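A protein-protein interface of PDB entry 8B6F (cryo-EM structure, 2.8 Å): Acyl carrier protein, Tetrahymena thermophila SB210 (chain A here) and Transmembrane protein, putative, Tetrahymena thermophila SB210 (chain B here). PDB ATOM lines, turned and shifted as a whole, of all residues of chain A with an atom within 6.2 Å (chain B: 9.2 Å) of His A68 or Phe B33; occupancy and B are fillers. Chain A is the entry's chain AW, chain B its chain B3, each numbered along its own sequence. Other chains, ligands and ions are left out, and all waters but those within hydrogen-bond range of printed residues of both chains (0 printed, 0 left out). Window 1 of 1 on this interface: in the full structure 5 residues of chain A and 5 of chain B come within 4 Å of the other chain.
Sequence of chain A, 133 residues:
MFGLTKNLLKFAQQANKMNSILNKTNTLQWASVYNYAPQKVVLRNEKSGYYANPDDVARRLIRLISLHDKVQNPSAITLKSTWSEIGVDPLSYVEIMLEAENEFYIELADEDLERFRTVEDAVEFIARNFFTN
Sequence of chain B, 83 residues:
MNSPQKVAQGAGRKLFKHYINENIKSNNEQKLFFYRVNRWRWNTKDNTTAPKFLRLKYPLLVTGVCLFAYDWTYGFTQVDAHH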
ATOM      1  N   ARG A  63      17.987  -8.968 -22.776  1.00  0.00           N
ATOM      2  CA  ARG A  63      16.647  -9.353 -22.346  1.00  0.00           C
ATOM      3  C   ARG A  63      15.914 -10.079 -23.463  1.00  0.00           C
ATOM      4  O   ARG A  63      15.255 -11.096 -23.224  1.00  0.00           O
ATOM      5  CB  ARG A  63      15.855  -8.124 -21.903  1.00  0.00           C
ATOM      6  CG  ARG A  63      16.387  -7.445 -20.652  1.00  0.00           C
ATOM      7  CD  ARG A  63      15.410  -6.394 -20.147  1.00  0.00           C
ATOM      8  NE  ARG A  63      16.018  -5.491 -19.176  1.00  0.00           N
ATOM      9  CZ  ARG A  63      16.539  -4.307 -19.466  1.00  0.00           C
ATOM     10  NH1 ARG A  63      16.546  -3.835 -20.701  1.00  0.00           N
ATOM     11  NH2 ARG A  63      17.066  -3.574 -18.489  1.00  0.00           N
ATOM     12  N   LEU A  64      16.018  -9.575 -24.692  1.00  0.00           N
ATOM     13  CA  LEU A  64      15.375 -10.244 -25.815  1.00  0.00           C
ATOM     14  C   LEU A  64      15.921 -11.653 -25.991  1.00  0.00           C
ATOM     15  O   LEU A  64      15.162 -12.598 -26.233  1.00  0.00           O
ATOM     16  CB  LEU A  64      15.573  -9.429 -27.091  1.00  0.00           C
ATOM     17  CG  LEU A  64      14.926 -10.002 -28.353  1.00  0.00           C
ATOM     18  CD1 LEU A  64      13.414 -10.016 -28.234  1.00  0.00           C
ATOM     19  CD2 LEU A  64      15.359  -9.205 -29.564  1.00  0.00           C
ATOM     20  N   ILE A  65      17.241 -11.813 -25.877  1.00  0.00           N
ATOM     21  CA  ILE A  65      17.847 -13.135 -25.998  1.00  0.00           C
ATOM     22  C   ILE A  65      17.353 -14.048 -24.885  1.00  0.00           C
ATOM     23  O   ILE A  65      17.015 -15.214 -25.122  1.00  0.00           O
ATOM     24  CB  ILE A  65      19.383 -13.022 -26.003  1.00  0.00           C
ATOM     25  CG1 ILE A  65      19.859 -12.285 -27.253  1.00  0.00           C
ATOM     26  CG2 ILE A  65      20.029 -14.400 -25.942  1.00  0.00           C
ATOM     27  CD1 ILE A  65      21.288 -11.804 -27.166  1.00  0.00           C
ATOM     28  N   SER A  66      17.298 -13.535 -23.655  1.00  0.00           N
ATOM     29  CA  SER A  66      16.845 -14.356 -22.537  1.00  0.00           C
ATOM     30  C   SER A  66      15.397 -14.791 -22.705  1.00  0.00           C
ATOM     31  O   SER A  66      15.012 -15.859 -22.217  1.00  0.00           O
ATOM     32  CB  SER A  66      17.010 -13.581 -21.231  1.00  0.00           C
ATOM     33  OG  SER A  66      18.356 -13.188 -21.043  1.00  0.00           O
ATOM     34  N   LEU A  67      14.579 -13.982 -23.379  1.00  0.00           N
ATOM     35  CA  LEU A  67      13.189 -14.363 -23.603  1.00  0.00           C
ATOM     36  C   LEU A  67      13.076 -15.671 -24.378  1.00  0.00           C
ATOM     37  O   LEU A  67      12.072 -16.381 -24.247  1.00  0.00           O
ATOM     38  CB  LEU A  67      12.452 -13.248 -24.349  1.00  0.00           C
ATOM     39  CG  LEU A  67      12.113 -11.987 -23.553  1.00  0.00           C
ATOM     40  CD1 LEU A  67      11.447 -10.960 -24.451  1.00  0.00           C
ATOM     41  CD2 LEU A  67      11.228 -12.295 -22.359  1.00  0.00           C
ATOM     42  N   HIS A  68      14.082 -16.008 -25.178  1.00  0.00           N
ATOM     43  CA  HIS A  68      14.003 -17.191 -26.021  1.00  0.00           C
ATOM     44  C   HIS A  68      13.983 -18.460 -25.176  1.00  0.00           C
ATOM     45  O   HIS A  68      14.501 -18.500 -24.057  1.00  0.00           O
ATOM     46  CB  HIS A  68      15.179 -17.230 -26.996  1.00  0.00           C
ATOM     47  CG  HIS A  68      14.915 -18.038 -28.228  1.00  0.00           C
ATOM     48  ND1 HIS A  68      14.992 -19.413 -28.249  1.00  0.00           N
ATOM     49  CD2 HIS A  68      14.578 -17.662 -29.484  1.00  0.00           C
ATOM     50  CE1 HIS A  68      14.710 -19.849 -29.463  1.00  0.00           C
ATOM     51  NE2 HIS A  68      14.456 -18.807 -30.232  1.00  0.00           N
ATOM     52  N   ASP A  69      13.369 -19.509 -25.728  1.00  0.00           N
ATOM     53  CA  ASP A  69      13.226 -20.761 -24.991  1.00  0.00           C
ATOM     54  C   ASP A  69      14.552 -21.506 -24.885  1.00  0.00           C
ATOM     55  O   ASP A  69      14.874 -22.061 -23.829  1.00  0.00           O
ATOM     56  CB  ASP A  69      12.177 -21.643 -25.664  1.00  0.00           C
ATOM     57  CG  ASP A  69      10.817 -20.980 -25.731  1.00  0.00           C
ATOM     58  OD1 ASP A  69      10.483 -20.216 -24.804  1.00  0.00           O
ATOM     59  OD2 ASP A  69      10.085 -21.217 -26.713  1.00  0.00           O
ATOM     60  N   LYS A  70      15.328 -21.537 -25.971  1.00  0.00           N
ATOM     61  CA  LYS A  70      16.592 -22.265 -25.952  1.00  0.00           C
ATOM     62  C   LYS A  70      17.556 -21.691 -24.925  1.00  0.00           C
ATOM     63  O   LYS A  70      18.331 -22.438 -24.319  1.00  0.00           O
ATOM     64  CB  LYS A  70      17.226 -22.247 -27.343  1.00  0.00           C
ATOM     65  CG  LYS A  70      16.407 -22.960 -28.407  1.00  0.00           C
ATOM     66  CD  LYS A  70      16.327 -24.457 -28.146  1.00  0.00           C
ATOM     67  CE  LYS A  70      15.578 -25.169 -29.261  1.00  0.00           C
ATOM     68  NZ  LYS A  70      15.525 -26.642 -29.042  1.00  0.00           N
ATOM     69  N   VAL A  71      17.529 -20.376 -24.718  1.00  0.00           N
ATOM     70  CA  VAL A  71      18.398 -19.757 -23.727  1.00  0.00           C
ATOM     71  C   VAL A  71      17.986 -20.228 -22.341  1.00  0.00           C
ATOM     72  O   VAL A  71      16.811 -20.140 -21.960  1.00  0.00           O
ATOM     73  CB  VAL A  71      18.341 -18.227 -23.845  1.00  0.00           C
ATOM     74  CG1 VAL A  71      19.180 -17.567 -22.761  1.00  0.00           C
ATOM     75  CG2 VAL A  71      18.811 -17.793 -25.222  1.00  0.00           C
ATOM     76  N   GLN A  72      18.954 -20.730 -21.575  1.00  0.00           N
ATOM     77  CA  GLN A  72      18.696 -21.317 -20.267  1.00  0.00           C
ATOM     78  C   GLN A  72      19.074 -20.389 -19.119  1.00  0.00           C
ATOM     79  O   GLN A  72      18.248 -20.125 -18.240  1.00  0.00           O
ATOM     80  CB  GLN A  72      19.460 -22.641 -20.132  1.00  0.00           C
ATOM     81  CG  GLN A  72      19.136 -23.657 -21.217  1.00  0.00           C
ATOM     82  CD  GLN A  72      17.683 -24.084 -21.202  1.00  0.00           C
ATOM     83  OE1 GLN A  72      16.969 -23.867 -20.223  1.00  0.00           O
ATOM     84  NE2 GLN A  72      17.236 -24.696 -22.293  1.00  0.00           N
ATOM     85  N   SER A  92      17.749 -20.398 -34.441  1.00  0.00           N
ATOM     86  CA  SER A  92      17.214 -19.510 -33.415  1.00  0.00           C
ATOM     87  C   SER A  92      17.789 -18.109 -33.550  1.00  0.00           C
ATOM     88  O   SER A  92      17.152 -17.132 -33.139  1.00  0.00           O
ATOM     89  CB  SER A  92      17.511 -20.068 -32.024  1.00  0.00           C
ATOM     90  OG  SER A  92      16.950 -21.358 -31.862  1.00  0.00           O
ATOM     91  N   TYR A  93      18.988 -17.993 -34.119  1.00  0.00           N
ATOM     92  CA  TYR A  93      19.620 -16.687 -34.261  1.00  0.00           C
ATOM     93  C   TYR A  93      18.804 -15.768 -35.163  1.00  0.00           C
ATOM     94  O   TYR A  93      18.649 -14.577 -34.868  1.00  0.00           O
ATOM     95  CB  TYR A  93      21.038 -16.855 -34.804  1.00  0.00           C
ATOM     96  CG  TYR A  93      21.750 -15.550 -35.062  1.00  0.00           C
ATOM     97  CD1 TYR A  93      22.255 -14.793 -34.014  1.00  0.00           C
ATOM     98  CD2 TYR A  93      21.925 -15.080 -36.356  1.00  0.00           C
ATOM     99  CE1 TYR A  93      22.908 -13.600 -34.247  1.00  0.00           C
ATOM    100  CE2 TYR A  93      22.576 -13.888 -36.600  1.00  0.00           C
ATOM    101  CZ  TYR A  93      23.066 -13.152 -35.542  1.00  0.00           C
ATOM    102  OH  TYR A  93      23.718 -11.966 -35.778  1.00  0.00           O
ATOM    103  N   GLU A  95      15.570 -15.842 -35.762  1.00  0.00           N
ATOM    104  CA  GLU A  95      14.369 -15.421 -35.047  1.00  0.00           C
ATOM    105  C   GLU A  95      14.688 -14.310 -34.058  1.00  0.00           C
ATOM    106  O   GLU A  95      13.983 -13.298 -33.991  1.00  0.00           O
ATOM    107  CB  GLU A  95      13.747 -16.613 -34.320  1.00  0.00           C
ATOM    108  CG  GLU A  95      13.464 -17.807 -35.207  1.00  0.00           C
ATOM    109  CD  GLU A  95      13.086 -19.035 -34.408  1.00  0.00           C
ATOM    110  OE1 GLU A  95      13.022 -18.938 -33.166  1.00  0.00           O
ATOM    111  OE2 GLU A  95      12.857 -20.099 -35.020  1.00  0.00           O
ATOM    112  N   ILE A  96      15.751 -14.489 -33.272  1.00  0.00           N
ATOM    113  CA  ILE A  96      16.125 -13.480 -32.287  1.00  0.00           C
ATOM    114  C   ILE A  96      16.474 -12.170 -32.979  1.00  0.00           C
ATOM    115  O   ILE A  96      16.163 -11.083 -32.480  1.00  0.00           O
ATOM    116  CB  ILE A  96      17.284 -13.994 -31.415  1.00  0.00           C
ATOM    117  CG1 ILE A  96      16.819 -15.189 -30.580  1.00  0.00           C
ATOM    118  CG2 ILE A  96      17.813 -12.883 -30.514  1.00  0.00           C
ATOM    119  CD1 ILE A  96      17.931 -15.899 -29.836  1.00  0.00           C
ATOM    120  N   GLU A  99      13.289 -10.345 -34.175  1.00  0.00           N
ATOM    121  CA  GLU A  99      12.652  -9.664 -33.055  1.00  0.00           C
ATOM    122  C   GLU A  99      13.490  -8.490 -32.572  1.00  0.00           C
ATOM    123  O   GLU A  99      12.940  -7.494 -32.090  1.00  0.00           O
ATOM    124  CB  GLU A  99      12.391 -10.646 -31.914  1.00  0.00           C
ATOM    125  CG  GLU A  99      11.355 -11.709 -32.247  1.00  0.00           C
ATOM    126  CD  GLU A  99      10.060 -11.126 -32.786  1.00  0.00           C
ATOM    127  OE1 GLU A  99       9.712  -9.990 -32.407  1.00  0.00           O
ATOM    128  OE2 GLU A  99       9.395 -11.805 -33.597  1.00  0.00           O
ATOM    129  N   GLU B  29       3.817 -27.816 -28.842  1.00  0.00           N
ATOM    130  CA  GLU B  29       5.076 -27.676 -29.561  1.00  0.00           C
ATOM    131  C   GLU B  29       5.405 -26.229 -29.900  1.00  0.00           C
ATOM    132  O   GLU B  29       6.533 -25.953 -30.317  1.00  0.00           O
ATOM    133  CB  GLU B  29       5.049 -28.511 -30.841  1.00  0.00           C
ATOM    134  CG  GLU B  29       5.262 -29.999 -30.607  1.00  0.00           C
ATOM    135  CD  GLU B  29       5.306 -30.793 -31.898  1.00  0.00           C
ATOM    136  OE1 GLU B  29       5.153 -30.184 -32.977  1.00  0.00           O
ATOM    137  OE2 GLU B  29       5.491 -32.027 -31.832  1.00  0.00           O
ATOM    138  N   GLN B  30       4.461 -25.306 -29.737  1.00  0.00           N
ATOM    139  CA  GLN B  30       4.724 -23.913 -30.050  1.00  0.00           C
ATOM    140  C   GLN B  30       5.758 -23.327 -29.091  1.00  0.00           C
ATOM    141  O   GLN B  30       5.941 -23.796 -27.965  1.00  0.00           O
ATOM    142  CB  GLN B  30       3.436 -23.091 -29.969  1.00  0.00           C
ATOM    143  CG  GLN B  30       2.439 -23.389 -31.073  1.00  0.00           C
ATOM    144  CD  GLN B  30       1.241 -22.469 -31.046  1.00  0.00           C
ATOM    145  OE1 GLN B  30       1.062 -21.687 -30.114  1.00  0.00           O
ATOM    146  NE2 GLN B  30       0.422 -22.541 -32.088  1.00  0.00           N
ATOM    147  N   LYS B  31       6.441 -22.285 -29.559  1.00  0.00           N
ATOM    148  CA  LYS B  31       7.429 -21.571 -28.762  1.00  0.00           C
ATOM    149  C   LYS B  31       6.791 -20.355 -28.107  1.00  0.00           C
ATOM    150  O   LYS B  31       6.028 -19.622 -28.741  1.00  0.00           O
ATOM    151  CB  LYS B  31       8.616 -21.127 -29.621  1.00  0.00           C
ATOM    152  CG  LYS B  31       9.408 -22.268 -30.236  1.00  0.00           C
ATOM    153  CD  LYS B  31      10.619 -21.744 -30.993  1.00  0.00           C
ATOM    154  CE  LYS B  31      11.391 -22.871 -31.662  1.00  0.00           C
ATOM    155  NZ  LYS B  31      10.593 -23.551 -32.719  1.00  0.00           N
ATOM    156  N   LEU B  32       7.112 -20.143 -26.833  1.00  0.00           N
ATOM    157  CA  LEU B  32       6.593 -19.003 -26.091  1.00  0.00           C
ATOM    158  C   LEU B  32       7.366 -17.723 -26.365  1.00  0.00           C
ATOM    159  O   LEU B  32       6.971 -16.662 -25.872  1.00  0.00           O
ATOM    160  CB  LEU B  32       6.609 -19.302 -24.591  1.00  0.00           C
ATOM    161  CG  LEU B  32       5.763 -20.492 -24.134  1.00  0.00           C
ATOM    162  CD1 LEU B  32       5.926 -20.708 -22.641  1.00  0.00           C
ATOM    163  CD2 LEU B  32       4.296 -20.293 -24.487  1.00  0.00           C
ATOM    164  N   PHE B  33       8.451 -17.796 -27.136  1.00  0.00           N
ATOM    165  CA  PHE B  33       9.242 -16.608 -27.430  1.00  0.00           C
ATOM    166  C   PHE B  33       8.413 -15.566 -28.169  1.00  0.00           C
ATOM    167  O   PHE B  33       8.453 -14.374 -27.841  1.00  0.00           O
ATOM    168  CB  PHE B  33      10.473 -17.012 -28.244  1.00  0.00           C
ATOM    169  CG  PHE B  33      11.252 -15.856 -28.793  1.00  0.00           C
ATOM    170  CD1 PHE B  33      11.980 -15.030 -27.953  1.00  0.00           C
ATOM    171  CD2 PHE B  33      11.287 -15.618 -30.155  1.00  0.00           C
ATOM    172  CE1 PHE B  33      12.711 -13.975 -28.464  1.00  0.00           C
ATOM    173  CE2 PHE B  33      12.014 -14.567 -30.668  1.00  0.00           C
ATOM    174  CZ  PHE B  33      12.727 -13.744 -29.822  1.00  0.00           C
ATOM    175  N   PHE B  34       7.648 -15.998 -29.173  1.00  0.00           N
ATOM    176  CA  PHE B  34       6.835 -15.061 -29.943  1.00  0.00           C
ATOM    177  C   PHE B  34       5.731 -14.451 -29.089  1.00  0.00           C
ATOM    178  O   PHE B  34       5.447 -13.254 -29.194  1.00  0.00           O
ATOM    179  CB  PHE B  34       6.260 -15.757 -31.174  1.00  0.00           C
ATOM    180  CG  PHE B  34       7.310 -16.346 -32.064  1.00  0.00           C
ATOM    181  CD1 PHE B  34       8.104 -15.528 -32.849  1.00  0.00           C
ATOM    182  CD2 PHE B  34       7.512 -17.712 -32.109  1.00  0.00           C
ATOM    183  CE1 PHE B  34       9.077 -16.063 -33.667  1.00  0.00           C
ATOM    184  CE2 PHE B  34       8.483 -18.253 -32.925  1.00  0.00           C
ATOM    185  CZ  PHE B  34       9.267 -17.427 -33.705  1.00  0.00           C
ATOM    186  N   TYR B  35       5.082 -15.261 -28.252  1.00  0.00           N
ATOM    187  CA  TYR B  35       4.082 -14.727 -27.333  1.00  0.00           C
ATOM    188  C   TYR B  35       4.691 -13.678 -26.414  1.00  0.00           C
ATOM    189  O   TYR B  35       4.122 -12.599 -26.219  1.00  0.00           O
ATOM    190  CB  TYR B  35       3.468 -15.855 -26.506  1.00  0.00           C
ATOM    191  CG  TYR B  35       2.588 -16.795 -27.292  1.00  0.00           C
ATOM    192  CD1 TYR B  35       1.233 -16.542 -27.442  1.00  0.00           C
ATOM    193  CD2 TYR B  35       3.109 -17.944 -27.866  1.00  0.00           C
ATOM    194  CE1 TYR B  35       0.422 -17.400 -28.150  1.00  0.00           C
ATOM    195  CE2 TYR B  35       2.308 -18.809 -28.577  1.00  0.00           C
ATOM    196  CZ  TYR B  35       0.965 -18.532 -28.715  1.00  0.00           C
ATOM    197  OH  TYR B  35       0.161 -19.392 -29.425  1.00  0.00           O
ATOM    198  N   ARG B  36       5.866 -13.971 -25.857  1.00  0.00           N
ATOM    199  CA  ARG B  36       6.504 -13.048 -24.923  1.00  0.00           C
ATOM    200  C   ARG B  36       6.838 -11.718 -25.584  1.00  0.00           C
ATOM    201  O   ARG B  36       6.621 -10.655 -24.992  1.00  0.00           O
ATOM    202  CB  ARG B  36       7.767 -13.687 -24.348  1.00  0.00           C
ATOM    203  CG  ARG B  36       7.498 -14.867 -23.431  1.00  0.00           C
ATOM    204  CD  ARG B  36       8.739 -15.722 -23.255  1.00  0.00           C
ATOM    205  NE  ARG B  36       8.487 -16.868 -22.392  1.00  0.00           N
ATOM    206  CZ  ARG B  36       9.355 -17.842 -22.164  1.00  0.00           C
ATOM    207  NH1 ARG B  36      10.553 -17.846 -22.726  1.00  0.00           N
ATOM    208  NH2 ARG B  36       9.016 -18.837 -21.352  1.00  0.00           N
ATOM    209  N   VAL B  37       7.369 -11.750 -26.806  1.00  0.00           N
ATOM    210  CA  VAL B  37       7.746 -10.503 -27.464  1.00  0.00           C
ATOM    211  C   VAL B  37       6.516  -9.703 -27.882  1.00  0.00           C
ATOM    212  O   VAL B  37       6.557  -8.468 -27.907  1.00  0.00           O
ATOM    213  CB  VAL B  37       8.670 -10.781 -28.664  1.00  0.00           C
ATOM    214  CG1 VAL B  37       9.951 -11.452 -28.202  1.00  0.00           C
ATOM    215  CG2 VAL B  37       7.969 -11.633 -29.702  1.00  0.00           C
ATOM    216  N   ASN B  38       5.415 -10.371 -28.219  1.00  0.00           N
ATOM    217  CA  ASN B  38       4.228  -9.687 -28.717  1.00  0.00           C
ATOM    218  C   ASN B  38       3.195  -9.377 -27.638  1.00  0.00           C
ATOM    219  O   ASN B  38       2.160  -8.783 -27.955  1.00  0.00           O
ATOM    220  CB  ASN B  38       3.562 -10.529 -29.813  1.00  0.00           C
ATOM    221  CG  ASN B  38       4.339 -10.518 -31.111  1.00  0.00           C
ATOM    222  OD1 ASN B  38       4.258  -9.568 -31.887  1.00  0.00           O
ATOM    223  ND2 ASN B  38       5.083 -11.588 -31.366  1.00  0.00           N
ATOM    224  N   ARG B  39       3.438  -9.755 -26.380  1.00  0.00           N
ATOM    225  CA  ARG B  39       2.432  -9.539 -25.341  1.00  0.00           C
ATOM    226  C   ARG B  39       1.961  -8.091 -25.290  1.00  0.00           C
ATOM    227  O   ARG B  39       0.773  -7.825 -25.079  1.00  0.00           O
ATOM    228  CB  ARG B  39       2.973  -9.968 -23.976  1.00  0.00           C
ATOM    229  CG  ARG B  39       3.118 -11.472 -23.830  1.00  0.00           C
ATOM    230  CD  ARG B  39       2.720 -11.946 -22.444  1.00  0.00           C
ATOM    231  NE  ARG B  39       2.800 -13.397 -22.329  1.00  0.00           N
ATOM    232  CZ  ARG B  39       3.865 -14.067 -21.911  1.00  0.00           C
ATOM    233  NH1 ARG B  39       4.975 -13.447 -21.544  1.00  0.00           N
ATOM    234  NH2 ARG B  39       3.816 -15.394 -21.859  1.00  0.00           N
ATOM    235  N   TRP B  42      -1.491  -6.496 -27.263  1.00  0.00           N
ATOM    236  CA  TRP B  42      -2.893  -6.666 -26.904  1.00  0.00           C
ATOM    237  C   TRP B  42      -3.204  -6.149 -25.504  1.00  0.00           C
ATOM    238  O   TRP B  42      -4.073  -6.698 -24.819  1.00  0.00           O
ATOM    239  CB  TRP B  42      -3.286  -8.136 -27.033  1.00  0.00           C
ATOM    240  CG  TRP B  42      -2.650  -8.788 -28.214  1.00  0.00           C
ATOM    241  CD1 TRP B  42      -2.977  -8.609 -29.528  1.00  0.00           C
ATOM    242  CD2 TRP B  42      -1.566  -9.719 -28.192  1.00  0.00           C
ATOM    243  NE1 TRP B  42      -2.162  -9.377 -30.325  1.00  0.00           N
ATOM    244  CE2 TRP B  42      -1.288 -10.068 -29.527  1.00  0.00           C
ATOM    245  CE3 TRP B  42      -0.806 -10.294 -27.172  1.00  0.00           C
ATOM    246  CZ2 TRP B  42      -0.282 -10.965 -29.867  1.00  0.00           C
ATOM    247  CZ3 TRP B  42       0.192 -11.185 -27.509  1.00  0.00           C
ATOM    248  CH2 TRP B  42       0.446 -11.513 -28.846  1.00  0.00           C
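ND1 of His A68 lies within hydrogen-bond range of N of Lys A70 (3.1 Å). A ring nitrogen (NE2) of His A68 is in hydrogen-bond range of the side-chain carboxylate of Glu A95 (3.3 Å).
Hydrophobic or aromatic side chains of chain B that line the printed part of chain A: Leu B32, Phe B33 and Val B37. Of the 15 printed residues of chain A, 5 touch a printed residue of chain B. Among the printed residues, Asp or Glu carboxylates within 4 Å of a Lys or Arg side-chain nitrogen of the other chain: Asp A69 with Arg B36 (3.2 Å).
Leu A64 touches Phe B33 (O to CE1, 3.6 Å). CD1 of Leu A64 touches CG1 of Val B37, 3.7 Å away. Leu A67 touches Phe B33 (C to CD1, 3.8 Å). His A68 touches Phe B33 (CA to CD1, 3.5 Å). OD2 of Asp A69 touches CB of Lys B31, 3.3 Å away. N of Phe B33 touches OD2 of Asp A69 (3.8 Å). CG of Glu A99 touches CE2 of Phe B33, 3.3 Å away. Glu A99 touches Val B37 (OE1 to CG2, 3.6 Å).
His A68 touches one residue of chain B. Of chain A, only Leu A64, Leu A67, His A68, Asp A69 and Glu A99 come within 4 Å of Phe B33. Printed residues of chain B within 4 Å of Asp A69: Lys B31, Leu B32, Phe B33 and Arg B36. No residue of chain B comes within 4 Å of Val A71. Printed residues of chain B within 4 Å of Leu A67: Phe B33 and Arg B36. Printed residues of chain A within 4 Å of Leu B32: Asp A69. Printed residues of chain B within 4 Å of Glu A99: Phe B33 (3.3 Å) and Val B37 (3.6 Å). Of the printed residues of chain A, Val B37 touches Leu A64 (3.7 Å) and Glu A99 (3.6 Å). Of the printed residues of chain A, Arg B36 touches Leu A67 and Asp A69. Ser A92 touches none of the printed residues of chain B. Tyr B35 touches none of the printed residues of chain A. The nearest residue of chain A that does not touch Phe B33 is Glu A95 (4.1 Å). The nearest printed residue of chain A that does not touch Lys B31 is Glu A95 (4.3 Å).
O of Leu A67 is in hydrogen-bond range of NH1 of Arg B36 (2.6 Å). The side-chain carboxylate (OD1) of Asp A69 is in salt-bridge range of the guanidinium group (NH1) of Arg B36 (3.2 Å). The backbone NH of Leu B32 is in hydrogen-bond range of the side-chain carboxylate of Asp A69, at 3.2 Å.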
